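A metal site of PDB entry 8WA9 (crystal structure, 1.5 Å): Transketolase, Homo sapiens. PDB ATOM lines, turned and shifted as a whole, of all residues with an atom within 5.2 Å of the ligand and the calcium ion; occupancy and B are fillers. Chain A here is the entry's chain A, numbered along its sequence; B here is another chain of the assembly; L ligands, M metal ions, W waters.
The backbone NH (N) of Asp 155 sits close to an oxygen (O3) of the ligand (3.5 Å).
The side-chain amide oxygen (OE1) of Gln 428 of chain B lies within hydrogen-bond range of an oxygen (O8) of the ligand (2.5 Å).
An oxygen (O5) of the ligand lies within salt-bridge range of the side-chain amino group of Lys 75.
OG of Ser 40 is in hydrogen-bond range of O6 of the ligand.
A ring nitrogen (NE2) of His 77 lies within hydrogen-bond range of an oxygen (O6) of the ligand.
A nitrogen (N1) of the ligand sits at hydrogen-bond distance from the side-chain carboxylate (OE2) of Glu 366 of chain B, at 2.7 Å.
A ring nitrogen (NE2) of His 110 lies within hydrogen-bond range of an oxygen (O9) of the ligand.
O6 of the ligand lies within salt-bridge range of NZ of Lys 244 (3.2 Å).
The backbone NH of Glu 157 lies within hydrogen-bond range of an oxygen (O2) of the ligand (2.8 Å).
O2 of the ligand lies within hydrogen-bond range of N of Gly 156.
A nitrogen (N3) of the ligand sits at hydrogen-bond distance from the backbone carbonyl oxygen (O) of Gly 123 (2.9 Å).
The backbone NH of Leu 125 lies within hydrogen-bond range of a nitrogen (N2) of the ligand.
A nitrogen (N4) of the ligand lies close to the side-chain amide oxygen (OE1) of Gln 189 (3.3 Å).
A sulfur (S1) of the ligand sits close to a ring nitrogen (NE2) of His 258, 3.4 Å away.
NE2 of Gln 428 of chain B sits at hydrogen-bond distance from O of Gly 123, at 2.9 Å.
NZ of Lys 75 is in hydrogen-bond range of O of Ser 40, at 3.0 Å.
OG of Ser 43 is in hydrogen-bond range of O of Ser 40, 3.4 Å away.
OE1 of Glu 366 of chain B sits close to OE2 of Glu 160 (2.6 Å).
The backbone NH (N) of Gly 154 sits at hydrogen-bond distance from the side-chain carboxylate (OE1) of Glu 157 (2.8 Å).
OG of Ser 124 sits at hydrogen-bond distance from NH1 of Arg 395 of chain B (3.1 Å).
OG of Ser 124 lies within hydrogen-bond range of OD2 of Asp 398, 2.5 Å away.
The side-chain carboxylate (OD2) of Asp 398 lies within salt-bridge range of the guanidinium group (NH1) of Arg 395 of chain B (2.8 Å).
Residues that only touch the ligand: His 37, Ser 124, Gly 154, Glu 160, Gly 188, Asp 341 of chain B, Thr 342 of chain B, Ile 364 of chain B, Phe 389 of chain B, Phe 392 of chain B and Arg 395 of chain B.
Hydrophobic or aromatic side chains that line the ligand: His 77, His 110, Leu 125, His 258, Ile 364 of chain B, Phe 389 of chain B and Phe 392 of chain B.
Within 4 Å of the ligand: His 37, Ser 40, Lys 75, His 77, His 110, Gly 123, Ser 124, Leu 125, Gly 154, Asp 155, Gly 156, Glu 157, Glu 160, Asn 185, Leu 187, Gly 188, Gln 189, Lys 244, His 258, Asp 341 of chain B, Thr 342 of chain B, Ile 364 of chain B, Glu 366 of chain B, Phe 389 of chain B, Phe 392 of chain B, Arg 395 of chain B and Gln 428 of chain B.
The nearest printed residue that does not touch the ligand is Asp 183 (4.1 Å).
Of the 34 residues printed, 3 come within 4 Å of the calcium ion.
OD1 of Asp 155 binds the calcium ion (2.1 Å).
The calcium ion is bound by the backbone carbonyl oxygen (O) of Leu 187 (2.1 Å).
OD1 of Asn 185 is bound to the calcium ion, at 2.1 Å.
The calcium ion is bound by an oxygen (O3) of the ligand, at 2.2 Å.
The calcium ion is bound by an oxygen (O7) of the ligand, 2.2 Å away.
The calcium ion is bound by water W2, at 2.3 Å.
Water W2 lies within hydrogen-bond range of the backbone carbonyl oxygen of Asp 183, an oxygen (O5) of the ligand, the backbone NH of Asp 155 and the side-chain amide nitrogen of Asn 185.
Water W3 lies within hydrogen-bond range of O9 of the ligand, ND1 of His 77 and O of Gly 123.
Water W1 lies within hydrogen-bond range of the side-chain hydroxyl of Thr 388 of chain B, the backbone carbonyl oxygen of Gly 340 of chain B and the side-chain carboxylate of Glu 366 of chain B.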
ATOM      1  N   HIS A  37     -24.959  22.322   7.005  1.00  0.00           N
ATOM      2  CA  HIS A  37     -25.352  21.093   6.317  1.00  0.00           C
ATOM      3  C   HIS A  37     -26.380  21.402   5.228  1.00  0.00           C
ATOM      4  O   HIS A  37     -27.511  20.919   5.270  1.00  0.00           O
ATOM      5  CB  HIS A  37     -25.931  20.094   7.314  1.00  0.00           C
ATOM      6  CG  HIS A  37     -25.000  19.730   8.431  1.00  0.00           C
ATOM      7  ND1 HIS A  37     -24.696  20.601   9.449  1.00  0.00           N
ATOM      8  CD2 HIS A  37     -24.331  18.584   8.683  1.00  0.00           C
ATOM      9  CE1 HIS A  37     -23.860  20.004  10.293  1.00  0.00           C
ATOM     10  NE2 HIS A  37     -23.627  18.776   9.846  1.00  0.00           N
ATOM     11  N   SER A  40     -28.212  18.401   3.635  1.00  0.00           N
ATOM     12  CA  SER A  40     -29.221  17.786   4.494  1.00  0.00           C
ATOM     13  C   SER A  40     -30.483  18.621   4.536  1.00  0.00           C
ATOM     14  O   SER A  40     -31.573  18.095   4.776  1.00  0.00           O
ATOM     15  CB  SER A  40     -28.682  17.611   5.924  1.00  0.00           C
ATOM     16  OG  SER A  40     -27.459  16.886   5.939  1.00  0.00           O
ATOM     17  N   SER A  43     -32.598  18.004   0.858  1.00  0.00           N
ATOM     18  CA  SER A  43     -33.419  16.812   0.645  1.00  0.00           C
ATOM     19  C   SER A  43     -34.793  16.964   1.270  1.00  0.00           C
ATOM     20  O   SER A  43     -35.740  16.291   0.830  1.00  0.00           O
ATOM     21  CB  SER A  43     -32.726  15.564   1.207  1.00  0.00           C
ATOM     22  OG  SER A  43     -32.421  15.687   2.575  1.00  0.00           O
ATOM     23  N   LYS A  75     -33.733  15.323  12.859  1.00  0.00           N
ATOM     24  CA  LYS A  75     -32.438  15.501  12.200  1.00  0.00           C
ATOM     25  C   LYS A  75     -32.067  16.984  12.312  1.00  0.00           C
ATOM     26  O   LYS A  75     -32.165  17.768  11.362  1.00  0.00           O
ATOM     27  CB  LYS A  75     -32.479  15.005  10.762  1.00  0.00           C
ATOM     28  CG  LYS A  75     -33.725  15.416   9.965  1.00  0.00           C
ATOM     29  CD  LYS A  75     -33.566  15.063   8.487  1.00  0.00           C
ATOM     30  CE  LYS A  75     -32.848  16.197   7.735  1.00  0.00           C
ATOM     31  NZ  LYS A  75     -32.527  15.770   6.325  1.00  0.00           N
ATOM     32  N   HIS A  77     -29.469  18.819  12.515  1.00  0.00           N
ATOM     33  CA  HIS A  77     -28.481  19.510  11.694  1.00  0.00           C
ATOM     34  C   HIS A  77     -29.088  20.133  10.446  1.00  0.00           C
ATOM     35  O   HIS A  77     -28.390  20.882   9.743  1.00  0.00           O
ATOM     36  CB  HIS A  77     -27.348  18.556  11.314  1.00  0.00           C
ATOM     37  CG  HIS A  77     -27.808  17.311  10.633  1.00  0.00           C
ATOM     38  ND1 HIS A  77     -28.513  16.323  11.274  1.00  0.00           N
ATOM     39  CD2 HIS A  77     -27.656  16.893   9.350  1.00  0.00           C
ATOM     40  CE1 HIS A  77     -28.779  15.337  10.420  1.00  0.00           C
ATOM     41  NE2 HIS A  77     -28.281  15.671   9.247  1.00  0.00           N
ATOM     42  N   HIS A 110     -27.605  23.883  15.888  1.00  0.00           N
ATOM     43  CA  HIS A 110     -28.722  22.956  16.004  1.00  0.00           C
ATOM     44  C   HIS A 110     -29.813  23.616  16.825  1.00  0.00           C
ATOM     45  O   HIS A 110     -29.551  24.576  17.570  1.00  0.00           O
ATOM     46  CB  HIS A 110     -28.281  21.630  16.661  1.00  0.00           C
ATOM     47  CG  HIS A 110     -27.278  20.868  15.849  1.00  0.00           C
ATOM     48  ND1 HIS A 110     -25.939  21.217  15.822  1.00  0.00           N
ATOM     49  CD2 HIS A 110     -27.410  19.795  15.036  1.00  0.00           C
ATOM     50  CE1 HIS A 110     -25.293  20.383  15.024  1.00  0.00           C
ATOM     51  NE2 HIS A 110     -26.158  19.506  14.543  1.00  0.00           N
ATOM     52  N   GLY A 123     -29.958  17.307  17.787  1.00  0.00           N
ATOM     53  CA  GLY A 123     -28.556  17.388  17.430  1.00  0.00           C
ATOM     54  C   GLY A 123     -27.909  16.065  17.748  1.00  0.00           C
ATOM     55  O   GLY A 123     -27.014  15.616  17.039  1.00  0.00           O
ATOM     56  N   SER A 124     -28.377  15.421  18.819  1.00  0.00           N
ATOM     57  CA  SER A 124     -28.047  14.017  19.053  1.00  0.00           C
ATOM     58  C   SER A 124     -29.141  13.196  18.382  1.00  0.00           C
ATOM     59  O   SER A 124     -30.304  13.218  18.814  1.00  0.00           O
ATOM     60  CB  SER A 124     -27.944  13.688  20.528  1.00  0.00           C
ATOM     61  OG  SER A 124     -27.781  12.287  20.646  1.00  0.00           O
ATOM     62  N   LEU A 125     -28.771  12.487  17.328  1.00  0.00           N
ATOM     63  CA  LEU A 125     -29.759  11.880  16.441  1.00  0.00           C
ATOM     64  C   LEU A 125     -30.533  10.784  17.153  1.00  0.00           C
ATOM     65  O   LEU A 125     -30.042  10.115  18.074  1.00  0.00           O
ATOM     66  CB  LEU A 125     -29.072  11.294  15.210  1.00  0.00           C
ATOM     67  CG  LEU A 125     -28.536  12.369  14.267  1.00  0.00           C
ATOM     68  CD1 LEU A 125     -27.530  11.762  13.318  1.00  0.00           C
ATOM     69  CD2 LEU A 125     -29.676  12.998  13.512  1.00  0.00           C
ATOM     70  N   GLY A 154     -33.893  11.674   9.699  1.00  0.00           N
ATOM     71  CA  GLY A 154     -33.035  11.251   8.612  1.00  0.00           C
ATOM     72  C   GLY A 154     -33.021   9.740   8.459  1.00  0.00           C
ATOM     73  O   GLY A 154     -33.571   9.024   9.299  1.00  0.00           O
ATOM     74  N   ASP A 155     -32.383   9.247   7.392  1.00  0.00           N
ATOM     75  CA  ASP A 155     -32.376   7.790   7.237  1.00  0.00           C
ATOM     76  C   ASP A 155     -31.201   7.129   7.972  1.00  0.00           C
ATOM     77  O   ASP A 155     -31.403   6.085   8.613  1.00  0.00           O
ATOM     78  CB  ASP A 155     -32.452   7.341   5.750  1.00  0.00           C
ATOM     79  CG  ASP A 155     -31.398   7.944   4.835  1.00  0.00           C
ATOM     80  OD1 ASP A 155     -30.658   8.835   5.232  1.00  0.00           O
ATOM     81  OD2 ASP A 155     -31.339   7.487   3.667  1.00  0.00           O
ATOM     82  N   GLY A 156     -30.012   7.732   7.962  1.00  0.00           N
ATOM     83  CA  GLY A 156     -28.959   7.237   8.839  1.00  0.00           C
ATOM     84  C   GLY A 156     -29.404   7.239  10.292  1.00  0.00           C
ATOM     85  O   GLY A 156     -29.119   6.297  11.043  1.00  0.00           O
ATOM     86  N   GLU A 157     -30.151   8.277  10.684  1.00  0.00           N
ATOM     87  CA  GLU A 157     -30.696   8.403  12.030  1.00  0.00           C
ATOM     88  C   GLU A 157     -31.511   7.187  12.450  1.00  0.00           C
ATOM     89  O   GLU A 157     -31.547   6.853  13.648  1.00  0.00           O
ATOM     90  CB  GLU A 157     -31.555   9.664  12.082  1.00  0.00           C
ATOM     91  CG  GLU A 157     -32.272   9.874  13.406  1.00  0.00           C
ATOM     92  CD  GLU A 157     -32.925  11.220  13.512  1.00  0.00           C
ATOM     93  OE1 GLU A 157     -33.277  11.812  12.476  1.00  0.00           O
ATOM     94  OE2 GLU A 157     -33.085  11.690  14.651  1.00  0.00           O
ATOM     95  N   GLU A 160     -30.522   4.380  15.030  1.00  0.00           N
ATOM     96  CA  GLU A 160     -30.535   4.491  16.485  1.00  0.00           C
ATOM     97  C   GLU A 160     -31.657   3.669  17.068  1.00  0.00           C
ATOM     98  O   GLU A 160     -32.822   3.838  16.676  1.00  0.00           O
ATOM     99  CB  GLU A 160     -30.691   5.943  16.935  1.00  0.00           C
ATOM    100  CG  GLU A 160     -29.453   6.801  16.713  1.00  0.00           C
ATOM    101  CD  GLU A 160     -28.306   6.516  17.676  1.00  0.00           C
ATOM    102  OE1 GLU A 160     -28.377   5.596  18.505  1.00  0.00           O
ATOM    103  OE2 GLU A 160     -27.303   7.234  17.577  1.00  0.00           O
ATOM    104  N   ASP A 183     -36.776  11.079   5.850  1.00  0.00           N
ATOM    105  CA  ASP A 183     -36.053  11.686   4.731  1.00  0.00           C
ATOM    106  C   ASP A 183     -35.055  10.652   4.225  1.00  0.00           C
ATOM    107  O   ASP A 183     -33.882  10.617   4.606  1.00  0.00           O
ATOM    108  CB  ASP A 183     -35.380  12.975   5.198  1.00  0.00           C
ATOM    109  CG  ASP A 183     -34.675  13.730   4.080  1.00  0.00           C
ATOM    110  OD1 ASP A 183     -34.617  13.254   2.925  1.00  0.00           O
ATOM    111  OD2 ASP A 183     -34.182  14.846   4.403  1.00  0.00           O
ATOM    112  N   ASN A 185     -32.834   9.982   1.977  1.00  0.00           N
ATOM    113  CA  ASN A 185     -31.990  10.569   0.950  1.00  0.00           C
ATOM    114  C   ASN A 185     -30.750   9.720   0.645  1.00  0.00           C
ATOM    115  O   ASN A 185     -29.812  10.223   0.007  1.00  0.00           O
ATOM    116  CB  ASN A 185     -31.594  12.006   1.333  1.00  0.00           C
ATOM    117  CG  ASN A 185     -30.749  12.095   2.585  1.00  0.00           C
ATOM    118  OD1 ASN A 185     -30.182  11.107   3.056  1.00  0.00           O
ATOM    119  ND2 ASN A 185     -30.662  13.298   3.128  1.00  0.00           N
ATOM    120  N   ARG A 186     -30.744   8.463   1.109  1.00  0.00           N
ATOM    121  CA  ARG A 186     -29.809   7.419   0.673  1.00  0.00           C
ATOM    122  C   ARG A 186     -28.490   7.451   1.429  1.00  0.00           C
ATOM    123  O   ARG A 186     -27.829   6.413   1.569  1.00  0.00           O
ATOM    124  CB  ARG A 186     -29.530   7.487  -0.840  1.00  0.00           C
ATOM    125  CG  ARG A 186     -28.926   6.195  -1.379  1.00  0.00           C
ATOM    126  CD  ARG A 186     -28.699   6.224  -2.911  1.00  0.00           C
ATOM    127  NE  ARG A 186     -27.694   7.207  -3.309  1.00  0.00           N
ATOM    128  CZ  ARG A 186     -26.386   7.002  -3.266  1.00  0.00           C
ATOM    129  NH1 ARG A 186     -25.877   5.858  -2.802  1.00  0.00           N
ATOM    130  NH2 ARG A 186     -25.561   7.955  -3.688  1.00  0.00           N
ATOM    131  N   LEU A 187     -28.095   8.618   1.925  1.00  0.00           N
ATOM    132  CA  LEU A 187     -26.740   8.840   2.421  1.00  0.00           C
ATOM    133  C   LEU A 187     -26.766   9.255   3.882  1.00  0.00           C
ATOM    134  O   LEU A 187     -27.654  10.003   4.307  1.00  0.00           O
ATOM    135  CB  LEU A 187     -26.015   9.920   1.600  1.00  0.00           C
ATOM    136  CG  LEU A 187     -25.856   9.633   0.106  1.00  0.00           C
ATOM    137  CD1 LEU A 187     -25.152  10.790  -0.621  1.00  0.00           C
ATOM    138  CD2 LEU A 187     -25.093   8.321  -0.068  1.00  0.00           C
ATOM    139  N   GLY A 188     -25.804   8.772   4.649  1.00  0.00           N
ATOM    140  CA  GLY A 188     -25.505   9.313   5.968  1.00  0.00           C
ATOM    141  C   GLY A 188     -24.377  10.317   5.907  1.00  0.00           C
ATOM    142  O   GLY A 188     -24.254  11.067   4.935  1.00  0.00           O
ATOM    143  N   GLN A 189     -23.545  10.330   6.947  1.00  0.00           N
ATOM    144  CA  GLN A 189     -22.475  11.320   6.999  1.00  0.00           C
ATOM    145  C   GLN A 189     -21.259  10.889   6.198  1.00  0.00           C
ATOM    146  O   GLN A 189     -20.686  11.701   5.464  1.00  0.00           O
ATOM    147  CB  GLN A 189     -22.054  11.588   8.452  1.00  0.00           C
ATOM    148  CG  GLN A 189     -20.693  12.287   8.545  1.00  0.00           C
ATOM    149  CD  GLN A 189     -20.454  12.890   9.897  1.00  0.00           C
ATOM    150  OE1 GLN A 189     -21.381  13.394  10.535  1.00  0.00           O
ATOM    151  NE2 GLN A 189     -19.203  12.846  10.368  1.00  0.00           N
ATOM    152  N   LYS A 244     -30.066  13.534  -1.416  1.00  0.00           N
ATOM    153  CA  LYS A 244     -29.317  14.481  -0.601  1.00  0.00           C
ATOM    154  C   LYS A 244     -28.778  15.582  -1.506  1.00  0.00           C
ATOM    155  O   LYS A 244     -28.329  15.329  -2.631  1.00  0.00           O
ATOM    156  CB  LYS A 244     -28.177  13.766   0.126  1.00  0.00           C
ATOM    157  CG  LYS A 244     -27.715  14.484   1.412  1.00  0.00           C
ATOM    158  CD  LYS A 244     -26.946  13.534   2.333  1.00  0.00           C
ATOM    159  CE  LYS A 244     -26.539  14.234   3.618  1.00  0.00           C
ATOM    160  NZ  LYS A 244     -26.168  13.221   4.652  1.00  0.00           N
ATOM    161  N   HIS A 258     -21.613  15.746   3.133  1.00  0.00           N
ATOM    162  CA  HIS A 258     -22.330  15.926   4.390  1.00  0.00           C
ATOM    163  C   HIS A 258     -21.626  16.961   5.268  1.00  0.00           C
ATOM    164  O   HIS A 258     -20.431  16.849   5.554  1.00  0.00           O
ATOM    165  CB  HIS A 258     -22.448  14.613   5.163  1.00  0.00           C
ATOM    166  CG  HIS A 258     -23.178  14.768   6.463  1.00  0.00           C
ATOM    167  ND1 HIS A 258     -24.547  14.673   6.572  1.00  0.00           N
ATOM    168  CD2 HIS A 258     -22.726  15.070   7.707  1.00  0.00           C
ATOM    169  CE1 HIS A 258     -24.910  14.872   7.825  1.00  0.00           C
ATOM    170  NE2 HIS A 258     -23.826  15.137   8.535  1.00  0.00           N
ATOM    171  N   ASP A 398     -27.639  10.133  27.304  1.00  0.00           N
ATOM    172  CA  ASP A 398     -27.674  11.113  26.213  1.00  0.00           C
ATOM    173  C   ASP A 398     -29.028  11.820  26.154  1.00  0.00           C
ATOM    174  O   ASP A 398     -29.101  13.027  25.851  1.00  0.00           O
ATOM    175  CB  ASP A 398     -27.367  10.389  24.900  1.00  0.00           C
ATOM    176  CG  ASP A 398     -27.029  11.333  23.741  1.00  0.00           C
ATOM    177  OD1 ASP A 398     -26.699  12.515  23.961  1.00  0.00           O
ATOM    178  OD2 ASP A 398     -27.070  10.851  22.582  1.00  0.00           O
ATOM    179  N   GLY B 340     -19.007   5.002  14.381  1.00  0.00           N
ATOM    180  CA  GLY B 340     -20.437   5.142  14.147  1.00  0.00           C
ATOM    181  C   GLY B 340     -20.833   6.224  13.157  1.00  0.00           C
ATOM    182  O   GLY B 340     -21.437   7.230  13.529  1.00  0.00           O
ATOM    183  N   ASP B 341     -20.495   6.000  11.884  1.00  0.00           N
ATOM    184  CA  ASP B 341     -20.745   6.924  10.770  1.00  0.00           C
ATOM    185  C   ASP B 341     -20.090   8.273  11.009  1.00  0.00           C
ATOM    186  O   ASP B 341     -20.543   9.292  10.500  1.00  0.00           O
ATOM    187  CB  ASP B 341     -22.240   7.093  10.482  1.00  0.00           C
ATOM    188  CG  ASP B 341     -22.525   7.808   9.162  1.00  0.00           C
ATOM    189  OD1 ASP B 341     -21.709   7.688   8.219  1.00  0.00           O
ATOM    190  OD2 ASP B 341     -23.574   8.473   9.063  1.00  0.00           O
ATOM    191  N   THR B 342     -19.008   8.306  11.792  1.00  0.00           N
ATOM    192  CA  THR B 342     -18.292   9.563  12.002  1.00  0.00           C
ATOM    193  C   THR B 342     -16.823   9.453  11.605  1.00  0.00           C
ATOM    194  O   THR B 342     -16.022  10.282  12.040  1.00  0.00           O
ATOM    195  CB  THR B 342     -18.423  10.042  13.459  1.00  0.00           C
ATOM    196  OG1 THR B 342     -18.075   8.999  14.372  1.00  0.00           O
ATOM    197  CG2 THR B 342     -19.847  10.487  13.750  1.00  0.00           C
ATOM    198  N   ILE B 364     -25.068   4.685  12.880  1.00  0.00           N
ATOM    199  CA  ILE B 364     -25.398   5.670  13.932  1.00  0.00           C
ATOM    200  C   ILE B 364     -26.121   4.884  15.028  1.00  0.00           C
ATOM    201  O   ILE B 364     -27.352   4.865  15.150  1.00  0.00           O
ATOM    202  CB  ILE B 364     -26.220   6.842  13.393  1.00  0.00           C
ATOM    203  CG1 ILE B 364     -25.507   7.475  12.177  1.00  0.00           C
ATOM    204  CG2 ILE B 364     -26.403   7.887  14.447  1.00  0.00           C
ATOM    205  CD1 ILE B 364     -26.301   8.631  11.512  1.00  0.00           C
ATOM    206  N   GLU B 366     -24.456   3.966  18.705  1.00  0.00           N
ATOM    207  CA  GLU B 366     -23.337   3.933  19.636  1.00  0.00           C
ATOM    208  C   GLU B 366     -23.475   2.830  20.672  1.00  0.00           C
ATOM    209  O   GLU B 366     -22.471   2.229  21.081  1.00  0.00           O
ATOM    210  CB  GLU B 366     -23.194   5.287  20.335  1.00  0.00           C
ATOM    211  CG  GLU B 366     -22.894   6.446  19.392  1.00  0.00           C
ATOM    212  CD  GLU B 366     -24.106   6.951  18.620  1.00  0.00           C
ATOM    213  OE1 GLU B 366     -25.272   6.654  19.025  1.00  0.00           O
ATOM    214  OE2 GLU B 366     -23.890   7.675  17.621  1.00  0.00           O
ATOM    215  N   THR B 388     -16.290   7.837  18.107  1.00  0.00           N
ATOM    216  CA  THR B 388     -17.392   8.732  17.734  1.00  0.00           C
ATOM    217  C   THR B 388     -17.080  10.069  18.412  1.00  0.00           C
ATOM    218  O   THR B 388     -15.991  10.233  18.985  1.00  0.00           O
ATOM    219  CB  THR B 388     -18.769   8.168  18.126  1.00  0.00           C
ATOM    220  OG1 THR B 388     -19.789   9.084  17.731  1.00  0.00           O
ATOM    221  CG2 THR B 388     -18.885   7.948  19.643  1.00  0.00           C
ATOM    222  N   PHE B 389     -17.999  11.033  18.324  1.00  0.00           N
ATOM    223  CA  PHE B 389     -17.861  12.215  19.160  1.00  0.00           C
ATOM    224  C   PHE B 389     -17.988  11.796  20.618  1.00  0.00           C
ATOM    225  O   PHE B 389     -18.861  10.988  20.966  1.00  0.00           O
ATOM    226  CB  PHE B 389     -18.963  13.243  18.870  1.00  0.00           C
ATOM    227  CG  PHE B 389     -18.889  13.926  17.534  1.00  0.00           C
ATOM    228  CD1 PHE B 389     -18.345  13.307  16.409  1.00  0.00           C
ATOM    229  CD2 PHE B 389     -19.416  15.194  17.390  1.00  0.00           C
ATOM    230  CE1 PHE B 389     -18.321  13.970  15.184  1.00  0.00           C
ATOM    231  CE2 PHE B 389     -19.401  15.846  16.165  1.00  0.00           C
ATOM    232  CZ  PHE B 389     -18.850  15.231  15.061  1.00  0.00           C
ATOM    233  N   PHE B 392     -21.430  11.614  22.100  1.00  0.00           N
ATOM    234  CA  PHE B 392     -22.326  10.495  21.795  1.00  0.00           C
ATOM    235  C   PHE B 392     -21.913   9.205  22.493  1.00  0.00           C
ATOM    236  O   PHE B 392     -22.674   8.215  22.440  1.00  0.00           O
ATOM    237  CB  PHE B 392     -22.432  10.326  20.271  1.00  0.00           C
ATOM    238  CG  PHE B 392     -22.839  11.603  19.592  1.00  0.00           C
ATOM    239  CD1 PHE B 392     -23.810  12.408  20.161  1.00  0.00           C
ATOM    240  CD2 PHE B 392     -22.216  12.034  18.412  1.00  0.00           C
ATOM    241  CE1 PHE B 392     -24.173  13.610  19.571  1.00  0.00           C
ATOM    242  CE2 PHE B 392     -22.593  13.248  17.825  1.00  0.00           C
ATOM    243  CZ  PHE B 392     -23.569  14.029  18.414  1.00  0.00           C
ATOM    244  N   ARG B 395     -24.520   8.175  24.919  1.00  0.00           N
ATOM    245  CA  ARG B 395     -25.570   7.301  24.438  1.00  0.00           C
ATOM    246  C   ARG B 395     -25.321   5.857  24.850  1.00  0.00           C
ATOM    247  O   ARG B 395     -26.286   5.087  24.969  1.00  0.00           O
ATOM    248  CB  ARG B 395     -25.670   7.399  22.915  1.00  0.00           C
ATOM    249  CG  ARG B 395     -26.908   6.791  22.272  1.00  0.00           C
ATOM    250  CD  ARG B 395     -28.198   7.395  22.812  1.00  0.00           C
ATOM    251  NE  ARG B 395     -29.256   7.346  21.803  1.00  0.00           N
ATOM    252  CZ  ARG B 395     -29.410   8.264  20.863  1.00  0.00           C
ATOM    253  NH1 ARG B 395     -28.611   9.311  20.788  1.00  0.00           N
ATOM    254  NH2 ARG B 395     -30.379   8.111  19.957  1.00  0.00           N
ATOM    255  N   ASP B 424     -21.070  24.145  15.908  1.00  0.00           N
ATOM    256  CA  ASP B 424     -22.137  23.144  15.990  1.00  0.00           C
ATOM    257  C   ASP B 424     -23.011  23.349  17.225  1.00  0.00           C
ATOM    258  O   ASP B 424     -24.199  23.016  17.193  1.00  0.00           O
ATOM    259  CB  ASP B 424     -21.549  21.735  15.979  1.00  0.00           C
ATOM    260  CG  ASP B 424     -21.501  21.113  14.598  1.00  0.00           C
ATOM    261  OD1 ASP B 424     -21.973  21.726  13.613  1.00  0.00           O
ATOM    262  OD2 ASP B 424     -20.978  19.985  14.504  1.00  0.00           O
ATOM    263  N   GLN B 428     -23.326  18.728  20.210  1.00  0.00           N
ATOM    264  CA  GLN B 428     -22.137  18.017  19.781  1.00  0.00           C
ATOM    265  C   GLN B 428     -20.975  18.162  20.743  1.00  0.00           C
ATOM    266  O   GLN B 428     -19.920  17.581  20.491  1.00  0.00           O
ATOM    267  CB  GLN B 428     -21.691  18.505  18.398  1.00  0.00           C
ATOM    268  CG  GLN B 428     -22.831  18.783  17.434  1.00  0.00           C
ATOM    269  CD  GLN B 428     -23.517  17.524  16.971  1.00  0.00           C
ATOM    270  OE1 GLN B 428     -22.881  16.599  16.460  1.00  0.00           O
ATOM    271  NE2 GLN B 428     -24.831  17.475  17.150  1.00  0.00           N
HETATM  272  N1  LIG L   1     -24.476  10.147  16.630  1.00  0.00           N
HETATM  273  C1  LIG L   1     -25.471  10.905  17.090  1.00  0.00           C
HETATM  274  C2  LIG L   1     -26.311  10.232  18.246  1.00  0.00           C
HETATM  275  N2  LIG L   1     -25.842  12.070  16.691  1.00  0.00           N
HETATM  276  C3  LIG L   1     -25.015  12.551  15.706  1.00  0.00           C
HETATM  277  N3  LIG L   1     -25.444  13.835  15.445  1.00  0.00           N
HETATM  278  C4  LIG L   1     -23.998  11.829  15.203  1.00  0.00           C
HETATM  279  C5  LIG L   1     -23.687  10.651  15.630  1.00  0.00           C
HETATM  280  C6  LIG L   1     -23.035  12.415  14.168  1.00  0.00           C
HETATM  281  N4  LIG L   1     -23.706  12.868  12.885  1.00  0.00           N
HETATM  282  C7  LIG L   1     -24.336  14.124  12.746  1.00  0.00           C
HETATM  283  S1  LIG L   1     -25.428  14.154  11.347  1.00  0.00           S
HETATM  284  C8  LIG L   1     -25.005  12.487  10.890  1.00  0.00           C
HETATM  285  C9  LIG L   1     -24.082  11.986  11.889  1.00  0.00           C
HETATM  286  C10 LIG L   1     -23.483  10.706  11.766  1.00  0.00           C
HETATM  287  C11 LIG L   1     -25.441  11.777   9.709  1.00  0.00           C
HETATM  288  C12 LIG L   1     -26.985  12.002   9.681  1.00  0.00           C
HETATM  289  O1  LIG L   1     -27.332  11.233   8.527  1.00  0.00           O
HETATM  290  P1  LIG L   1     -28.892  11.129   8.244  1.00  0.00           P
HETATM  291  O2  LIG L   1     -29.739  10.754   9.404  1.00  0.00           O
HETATM  292  O3  LIG L   1     -29.084  10.271   7.114  1.00  0.00           O
HETATM  293  O4  LIG L   1     -29.434  12.605   7.912  1.00  0.00           O
HETATM  294  P2  LIG L   1     -29.237  13.489   6.500  1.00  0.00           P
HETATM  295  O5  LIG L   1     -30.582  14.053   6.242  1.00  0.00           O
HETATM  296  O6  LIG L   1     -28.198  14.540   6.811  1.00  0.00           O
HETATM  297  O7  LIG L   1     -28.765  12.596   5.418  1.00  0.00           O
HETATM  298  C13 LIG L   1     -23.875  15.459  13.235  1.00  0.00           C
HETATM  299  O8  LIG L   1     -22.761  15.488  14.271  1.00  0.00           O
HETATM  300  C14 LIG L   1     -24.523  16.739  13.035  1.00  0.00           C
HETATM  301  O9  LIG L   1     -25.589  16.846  14.141  1.00  0.00           O
HETATM  302 CA    CA M   1     -29.557  10.603   5.033  1.00  0.00          CA
HETATM  303  O   HOH W   1     -21.562   8.081  16.117  1.00  0.00           O
HETATM  304  O   HOH W   2     -31.525  11.521   5.650  1.00  0.00           O
HETATM  305  O   HOH W   3     -28.229  15.944  14.131  1.00  0.00           O
